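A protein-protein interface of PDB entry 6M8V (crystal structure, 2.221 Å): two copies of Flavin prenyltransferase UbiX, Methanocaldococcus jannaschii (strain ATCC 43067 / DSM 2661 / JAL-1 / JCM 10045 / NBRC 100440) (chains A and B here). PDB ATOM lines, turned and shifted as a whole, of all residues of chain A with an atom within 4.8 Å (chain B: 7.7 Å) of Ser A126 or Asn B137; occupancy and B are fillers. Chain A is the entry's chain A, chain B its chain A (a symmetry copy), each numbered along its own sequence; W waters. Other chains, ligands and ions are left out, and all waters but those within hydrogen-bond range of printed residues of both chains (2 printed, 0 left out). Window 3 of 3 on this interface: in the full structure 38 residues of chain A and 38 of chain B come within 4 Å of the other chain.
The backbone NH (N) of Ile A127 is in hydrogen-bond range of the side-chain amide oxygen (OD1) of Asn A125, 2.9 Å away. The side-chain amide oxygen of Asn A125 is in hydrogen-bond range of the backbone NH of His A128. O of Leu B133 lies close to OD1 of Asn B137.
Ser A126 touches three residues of chain B. Printed residues of chain B within 4 Å of Leu A129: Met B132 and Ser B136. Lys B134 touches none of the printed residues of chain A. Of the printed residues of chain A, Ser B136 touches Asn A125, Ser A126 and Leu A129. Asn B137 touches just one residue of chain A: Ser A126 (2.6 Å). Of the printed residues of chain A, Val B142 touches Phe A124. The nearest residue of chain B that does not touch Ser A126 is Met B132 (5.9 Å). The nearest printed residue of chain A that does not touch Asn B137 is Ile A127 (6.3 Å).
Of the 7 printed residues of chain A, 4 touch a printed residue of chain B. Hydrophobic or aromatic side chains of chain A within 4 Å of the printed part of chain B: Leu A129. Of the 15 printed residues of chain B, 5 touch a printed residue of chain A. Printed residues of chain B that touch a printed residue of chain A: Met B132, Leu B133, Ser B136, Asn B137 and Val B142. Among the printed residues, no Asp or Glu carboxylate lies within 4 Å of a Lys or Arg side-chain nitrogen of the other chain.
Water W2 lies within hydrogen-bond range of O of Phe A124, OG of Ser B136, N of Val B142 and O of Ala B140. Water W1 bridges N of Ser A126 and OG of Ser B136.
1 position is printed for both chains. Of the 7 pairs that touch across the chains among the printed residues, none has its exchanged pair printed and touching as well.
C of Asn A125 touches OG of Ser B136, at 3.9 Å. Ser A126 touches Leu B133 (O to CD1, 3.4 Å). Leu A129 touches Met B132. Ser B136 touches Leu A129.
The backbone NH of Phe A124 lies within hydrogen-bond range of the backbone carbonyl oxygen of Val B142 (3.2 Å). The side-chain hydroxyl (OG) of Ser B136 is in hydrogen-bond range of the side-chain hydroxyl (OG) of Ser A126 (3.0 Å). The side-chain amide nitrogen (ND2) of Asn B137 lies within hydrogen-bond range of the side-chain hydroxyl (OG) of Ser A126, at 2.6 Å.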
ATOM      1  N   PHE A 124     -13.650 -11.924  31.065  1.00  0.00           N
ATOM      2  CA  PHE A 124     -12.282 -12.167  30.623  1.00  0.00           C
ATOM      3  C   PHE A 124     -11.427 -10.937  30.905  1.00  0.00           C
ATOM      4  O   PHE A 124     -11.898  -9.800  30.806  1.00  0.00           O
ATOM      5  CB  PHE A 124     -12.232 -12.462  29.120  1.00  0.00           C
ATOM      6  CG  PHE A 124     -12.793 -13.802  28.725  1.00  0.00           C
ATOM      7  CD1 PHE A 124     -12.350 -14.966  29.329  1.00  0.00           C
ATOM      8  CD2 PHE A 124     -13.746 -13.894  27.723  1.00  0.00           C
ATOM      9  CE1 PHE A 124     -12.852 -16.199  28.954  1.00  0.00           C
ATOM     10  CE2 PHE A 124     -14.254 -15.124  27.342  1.00  0.00           C
ATOM     11  CZ  PHE A 124     -13.803 -16.279  27.958  1.00  0.00           C
ATOM     12  N   ASN A 125     -10.159 -11.166  31.250  1.00  0.00           N
ATOM     13  CA  ASN A 125      -9.189 -10.084  31.288  1.00  0.00           C
ATOM     14  C   ASN A 125      -8.342 -10.123  30.014  1.00  0.00           C
ATOM     15  O   ASN A 125      -8.525 -10.976  29.146  1.00  0.00           O
ATOM     16  CB  ASN A 125      -8.329 -10.144  32.559  1.00  0.00           C
ATOM     17  CG  ASN A 125      -7.468 -11.398  32.657  1.00  0.00           C
ATOM     18  OD1 ASN A 125      -6.962 -11.921  31.658  1.00  0.00           O
ATOM     19  ND2 ASN A 125      -7.277 -11.872  33.886  1.00  0.00           N
ATOM     20  N   SER A 126      -7.399  -9.184  29.905  1.00  0.00           N
ATOM     21  CA  SER A 126      -6.592  -9.073  28.694  1.00  0.00           C
ATOM     22  C   SER A 126      -5.652 -10.249  28.503  1.00  0.00           C
ATOM     23  O   SER A 126      -5.254 -10.529  27.368  1.00  0.00           O
ATOM     24  CB  SER A 126      -5.783  -7.783  28.720  1.00  0.00           C
ATOM     25  OG  SER A 126      -6.617  -6.686  28.401  1.00  0.00           O
ATOM     26  N   ILE A 127      -5.276 -10.929  29.582  1.00  0.00           N
ATOM     27  CA  ILE A 127      -4.422 -12.102  29.457  1.00  0.00           C
ATOM     28  C   ILE A 127      -5.187 -13.244  28.802  1.00  0.00           C
ATOM     29  O   ILE A 127      -4.690 -13.895  27.873  1.00  0.00           O
ATOM     30  CB  ILE A 127      -3.860 -12.495  30.836  1.00  0.00           C
ATOM     31  CG1 ILE A 127      -3.067 -11.314  31.413  1.00  0.00           C
ATOM     32  CG2 ILE A 127      -2.975 -13.719  30.718  1.00  0.00           C
ATOM     33  CD1 ILE A 127      -2.501 -11.544  32.793  1.00  0.00           C
ATOM     34  N   HIS A 128      -6.412 -13.501  29.272  1.00  0.00           N
ATOM     35  CA  HIS A 128      -7.260 -14.497  28.624  1.00  0.00           C
ATOM     36  C   HIS A 128      -7.446 -14.164  27.153  1.00  0.00           C
ATOM     37  O   HIS A 128      -7.289 -15.026  26.281  1.00  0.00           O
ATOM     38  CB  HIS A 128      -8.630 -14.568  29.316  1.00  0.00           C
ATOM     39  CG  HIS A 128      -8.557 -14.668  30.808  1.00  0.00           C
ATOM     40  ND1 HIS A 128      -9.487 -14.074  31.638  1.00  0.00           N
ATOM     41  CD2 HIS A 128      -7.681 -15.304  31.621  1.00  0.00           C
ATOM     42  CE1 HIS A 128      -9.179 -14.331  32.897  1.00  0.00           C
ATOM     43  NE2 HIS A 128      -8.086 -15.073  32.915  1.00  0.00           N
ATOM     44  N   LEU A 129      -7.788 -12.910  26.858  1.00  0.00           N
ATOM     45  CA  LEU A 129      -8.112 -12.542  25.484  1.00  0.00           C
ATOM     46  C   LEU A 129      -6.897 -12.680  24.572  1.00  0.00           C
ATOM     47  O   LEU A 129      -7.016 -13.153  23.437  1.00  0.00           O
ATOM     48  CB  LEU A 129      -8.675 -11.122  25.449  1.00  0.00           C
ATOM     49  CG  LEU A 129     -10.077 -11.030  26.067  1.00  0.00           C
ATOM     50  CD1 LEU A 129     -10.472  -9.590  26.401  1.00  0.00           C
ATOM     51  CD2 LEU A 129     -11.106 -11.655  25.122  1.00  0.00           C
ATOM     52  N   GLU A 130      -5.713 -12.301  25.053  1.00  0.00           N
ATOM     53  CA  GLU A 130      -4.523 -12.443  24.221  1.00  0.00           C
ATOM     54  C   GLU A 130      -4.144 -13.910  24.037  1.00  0.00           C
ATOM     55  O   GLU A 130      -3.658 -14.303  22.968  1.00  0.00           O
ATOM     56  CB  GLU A 130      -3.361 -11.658  24.824  1.00  0.00           C
ATOM     57  CG  GLU A 130      -2.242 -11.370  23.830  1.00  0.00           C
ATOM     58  CD  GLU A 130      -1.185 -12.461  23.805  1.00  0.00           C
ATOM     59  OE1 GLU A 130      -0.893 -13.025  24.881  1.00  0.00           O
ATOM     60  OE2 GLU A 130      -0.644 -12.750  22.715  1.00  0.00           O
ATOM     61  N   LEU B 109     -15.261   5.983  27.191  1.00  0.00           N
ATOM     62  CA  LEU B 109     -13.821   5.750  27.158  1.00  0.00           C
ATOM     63  C   LEU B 109     -13.044   7.055  27.304  1.00  0.00           C
ATOM     64  O   LEU B 109     -12.050   7.108  28.037  1.00  0.00           O
ATOM     65  CB  LEU B 109     -13.428   5.017  25.869  1.00  0.00           C
ATOM     66  CG  LEU B 109     -13.871   3.546  25.757  1.00  0.00           C
ATOM     67  CD1 LEU B 109     -13.755   3.014  24.328  1.00  0.00           C
ATOM     68  CD2 LEU B 109     -13.080   2.653  26.711  1.00  0.00           C
ATOM     69  N   ARG B 112     -13.480   8.318  30.829  1.00  0.00           N
ATOM     70  CA  ARG B 112     -13.030   7.335  31.816  1.00  0.00           C
ATOM     71  C   ARG B 112     -14.172   6.878  32.721  1.00  0.00           C
ATOM     72  O   ARG B 112     -14.013   6.746  33.933  1.00  0.00           O
ATOM     73  CB  ARG B 112     -11.861   7.871  32.643  1.00  0.00           C
ATOM     74  CG  ARG B 112     -10.688   8.362  31.818  1.00  0.00           C
ATOM     75  CD  ARG B 112     -10.026   7.243  30.994  1.00  0.00           C
ATOM     76  NE  ARG B 112      -8.801   7.733  30.355  1.00  0.00           N
ATOM     77  CZ  ARG B 112      -7.842   6.966  29.846  1.00  0.00           C
ATOM     78  NH1 ARG B 112      -7.938   5.641  29.877  1.00  0.00           N
ATOM     79  NH2 ARG B 112      -6.776   7.534  29.297  1.00  0.00           N
ATOM     80  N   GLU B 130      -9.457  -9.810  18.824  1.00  0.00           N
ATOM     81  CA  GLU B 130      -8.610  -8.622  18.849  1.00  0.00           C
ATOM     82  C   GLU B 130      -9.412  -7.372  19.201  1.00  0.00           C
ATOM     83  O   GLU B 130      -8.901  -6.468  19.875  1.00  0.00           O
ATOM     84  CB  GLU B 130      -7.904  -8.450  17.506  1.00  0.00           C
ATOM     85  CG  GLU B 130      -6.684  -7.539  17.574  1.00  0.00           C
ATOM     86  CD  GLU B 130      -7.027  -6.081  17.316  1.00  0.00           C
ATOM     87  OE1 GLU B 130      -7.915  -5.822  16.476  1.00  0.00           O
ATOM     88  OE2 GLU B 130      -6.407  -5.196  17.946  1.00  0.00           O
ATOM     89  N   ASN B 131     -10.659  -7.288  18.743  1.00  0.00           N
ATOM     90  CA  ASN B 131     -11.488  -6.144  19.116  1.00  0.00           C
ATOM     91  C   ASN B 131     -11.761  -6.147  20.615  1.00  0.00           C
ATOM     92  O   ASN B 131     -11.716  -5.098  21.264  1.00  0.00           O
ATOM     93  CB  ASN B 131     -12.795  -6.152  18.316  1.00  0.00           C
ATOM     94  CG  ASN B 131     -12.594  -5.743  16.863  1.00  0.00           C
ATOM     95  OD1 ASN B 131     -11.607  -5.093  16.530  1.00  0.00           O
ATOM     96  ND2 ASN B 131     -13.536  -6.112  15.997  1.00  0.00           N
ATOM     97  N   MET B 132     -12.004  -7.327  21.191  1.00  0.00           N
ATOM     98  CA  MET B 132     -12.195  -7.422  22.638  1.00  0.00           C
ATOM     99  C   MET B 132     -10.914  -7.107  23.397  1.00  0.00           C
ATOM    100  O   MET B 132     -10.945  -6.398  24.411  1.00  0.00           O
ATOM    101  CB  MET B 132     -12.704  -8.815  23.010  1.00  0.00           C
ATOM    102  CG  MET B 132     -14.145  -9.074  22.581  1.00  0.00           C
ATOM    103  SD  MET B 132     -14.770 -10.653  23.208  1.00  0.00           S
ATOM    104  CE  MET B 132     -14.444 -11.715  21.803  1.00  0.00           C
ATOM    105  N   LEU B 133      -9.780  -7.634  22.928  1.00  0.00           N
ATOM    106  CA  LEU B 133      -8.511  -7.382  23.600  1.00  0.00           C
ATOM    107  C   LEU B 133      -8.195  -5.892  23.637  1.00  0.00           C
ATOM    108  O   LEU B 133      -7.821  -5.349  24.687  1.00  0.00           O
ATOM    109  CB  LEU B 133      -7.393  -8.153  22.898  1.00  0.00           C
ATOM    110  CG  LEU B 133      -5.965  -7.923  23.393  1.00  0.00           C
ATOM    111  CD1 LEU B 133      -5.843  -8.285  24.878  1.00  0.00           C
ATOM    112  CD2 LEU B 133      -4.953  -8.712  22.537  1.00  0.00           C
ATOM    113  N   LYS B 134      -8.337  -5.214  22.496  1.00  0.00           N
ATOM    114  CA  LYS B 134      -8.105  -3.774  22.442  1.00  0.00           C
ATOM    115  C   LYS B 134      -8.948  -3.033  23.475  1.00  0.00           C
ATOM    116  O   LYS B 134      -8.442  -2.173  24.204  1.00  0.00           O
ATOM    117  CB  LYS B 134      -8.398  -3.243  21.035  1.00  0.00           C
ATOM    118  CG  LYS B 134      -8.140  -1.740  20.862  1.00  0.00           C
ATOM    119  CD  LYS B 134      -8.304  -1.325  19.402  1.00  0.00           C
ATOM    120  CE  LYS B 134      -8.329   0.180  19.230  1.00  0.00           C
ATOM    121  NZ  LYS B 134      -8.589   0.581  17.804  1.00  0.00           N
ATOM    122  N   LEU B 135     -10.238  -3.365  23.559  1.00  0.00           N
ATOM    123  CA  LEU B 135     -11.125  -2.654  24.476  1.00  0.00           C
ATOM    124  C   LEU B 135     -10.799  -2.986  25.925  1.00  0.00           C
ATOM    125  O   LEU B 135     -10.790  -2.097  26.782  1.00  0.00           O
ATOM    126  CB  LEU B 135     -12.582  -2.991  24.156  1.00  0.00           C
ATOM    127  CG  LEU B 135     -13.071  -2.348  22.852  1.00  0.00           C
ATOM    128  CD1 LEU B 135     -14.459  -2.851  22.453  1.00  0.00           C
ATOM    129  CD2 LEU B 135     -13.060  -0.844  22.998  1.00  0.00           C
ATOM    130  N   SER B 136     -10.514  -4.260  26.210  1.00  0.00           N
ATOM    131  CA  SER B 136     -10.061  -4.648  27.543  1.00  0.00           C
ATOM    132  C   SER B 136      -8.775  -3.924  27.925  1.00  0.00           C
ATOM    133  O   SER B 136      -8.616  -3.497  29.076  1.00  0.00           O
ATOM    134  CB  SER B 136      -9.866  -6.163  27.598  1.00  0.00           C
ATOM    135  OG  SER B 136      -9.576  -6.585  28.915  1.00  0.00           O
ATOM    136  N   ASN B 137      -7.845  -3.771  26.970  1.00  0.00           N
ATOM    137  CA  ASN B 137      -6.605  -3.038  27.236  1.00  0.00           C
ATOM    138  C   ASN B 137      -6.865  -1.577  27.562  1.00  0.00           C
ATOM    139  O   ASN B 137      -6.047  -0.941  28.237  1.00  0.00           O
ATOM    140  CB  ASN B 137      -5.656  -3.108  26.036  1.00  0.00           C
ATOM    141  CG  ASN B 137      -4.948  -4.441  25.924  1.00  0.00           C
ATOM    142  OD1 ASN B 137      -4.398  -4.772  24.877  1.00  0.00           O
ATOM    143  ND2 ASN B 137      -4.959  -5.211  26.996  1.00  0.00           N
ATOM    144  N   LEU B 138      -7.970  -1.017  27.069  1.00  0.00           N
ATOM    145  CA  LEU B 138      -8.324   0.369  27.351  1.00  0.00           C
ATOM    146  C   LEU B 138      -9.122   0.525  28.633  1.00  0.00           C
ATOM    147  O   LEU B 138      -9.468   1.654  28.991  1.00  0.00           O
ATOM    148  CB  LEU B 138      -9.121   0.965  26.186  1.00  0.00           C
ATOM    149  CG  LEU B 138      -8.351   1.055  24.869  1.00  0.00           C
ATOM    150  CD1 LEU B 138      -9.122   1.887  23.870  1.00  0.00           C
ATOM    151  CD2 LEU B 138      -6.950   1.614  25.089  1.00  0.00           C
ATOM    152  N   GLY B 139      -9.436  -0.573  29.323  1.00  0.00           N
ATOM    153  CA  GLY B 139     -10.136  -0.518  30.592  1.00  0.00           C
ATOM    154  C   GLY B 139     -11.593  -0.928  30.533  1.00  0.00           C
ATOM    155  O   GLY B 139     -12.250  -0.947  31.578  1.00  0.00           O
ATOM    156  N   ALA B 140     -12.128  -1.237  29.353  1.00  0.00           N
ATOM    157  CA  ALA B 140     -13.470  -1.789  29.280  1.00  0.00           C
ATOM    158  C   ALA B 140     -13.497  -3.176  29.911  1.00  0.00           C
ATOM    159  O   ALA B 140     -12.505  -3.904  29.894  1.00  0.00           O
ATOM    160  CB  ALA B 140     -13.947  -1.857  27.828  1.00  0.00           C
ATOM    161  N   ILE B 141     -14.643  -3.532  30.479  1.00  0.00           N
ATOM    162  CA  ILE B 141     -14.853  -4.845  31.074  1.00  0.00           C
ATOM    163  C   ILE B 141     -15.525  -5.726  30.029  1.00  0.00           C
ATOM    164  O   ILE B 141     -16.710  -5.560  29.728  1.00  0.00           O
ATOM    165  CB  ILE B 141     -15.682  -4.755  32.364  1.00  0.00           C
ATOM    166  CG1 ILE B 141     -14.922  -3.962  33.435  1.00  0.00           C
ATOM    167  CG2 ILE B 141     -16.003  -6.145  32.893  1.00  0.00           C
ATOM    168  CD1 ILE B 141     -15.518  -2.611  33.751  1.00  0.00           C
ATOM    169  N   VAL B 142     -14.772  -6.661  29.466  1.00  0.00           N
ATOM    170  CA  VAL B 142     -15.256  -7.495  28.373  1.00  0.00           C
ATOM    171  C   VAL B 142     -15.845  -8.757  28.986  1.00  0.00           C
ATOM    172  O   VAL B 142     -15.128  -9.572  29.574  1.00  0.00           O
ATOM    173  CB  VAL B 142     -14.141  -7.819  27.372  1.00  0.00           C
ATOM    174  CG1 VAL B 142     -14.655  -8.777  26.313  1.00  0.00           C
ATOM    175  CG2 VAL B 142     -13.619  -6.532  26.730  1.00  0.00           C
HETATM  176  O   HOH W   1      -7.470  -6.826  31.424  1.00  0.00           O
HETATM  177  O   HOH W   2     -12.050  -7.285  30.156  1.00  0.00           O
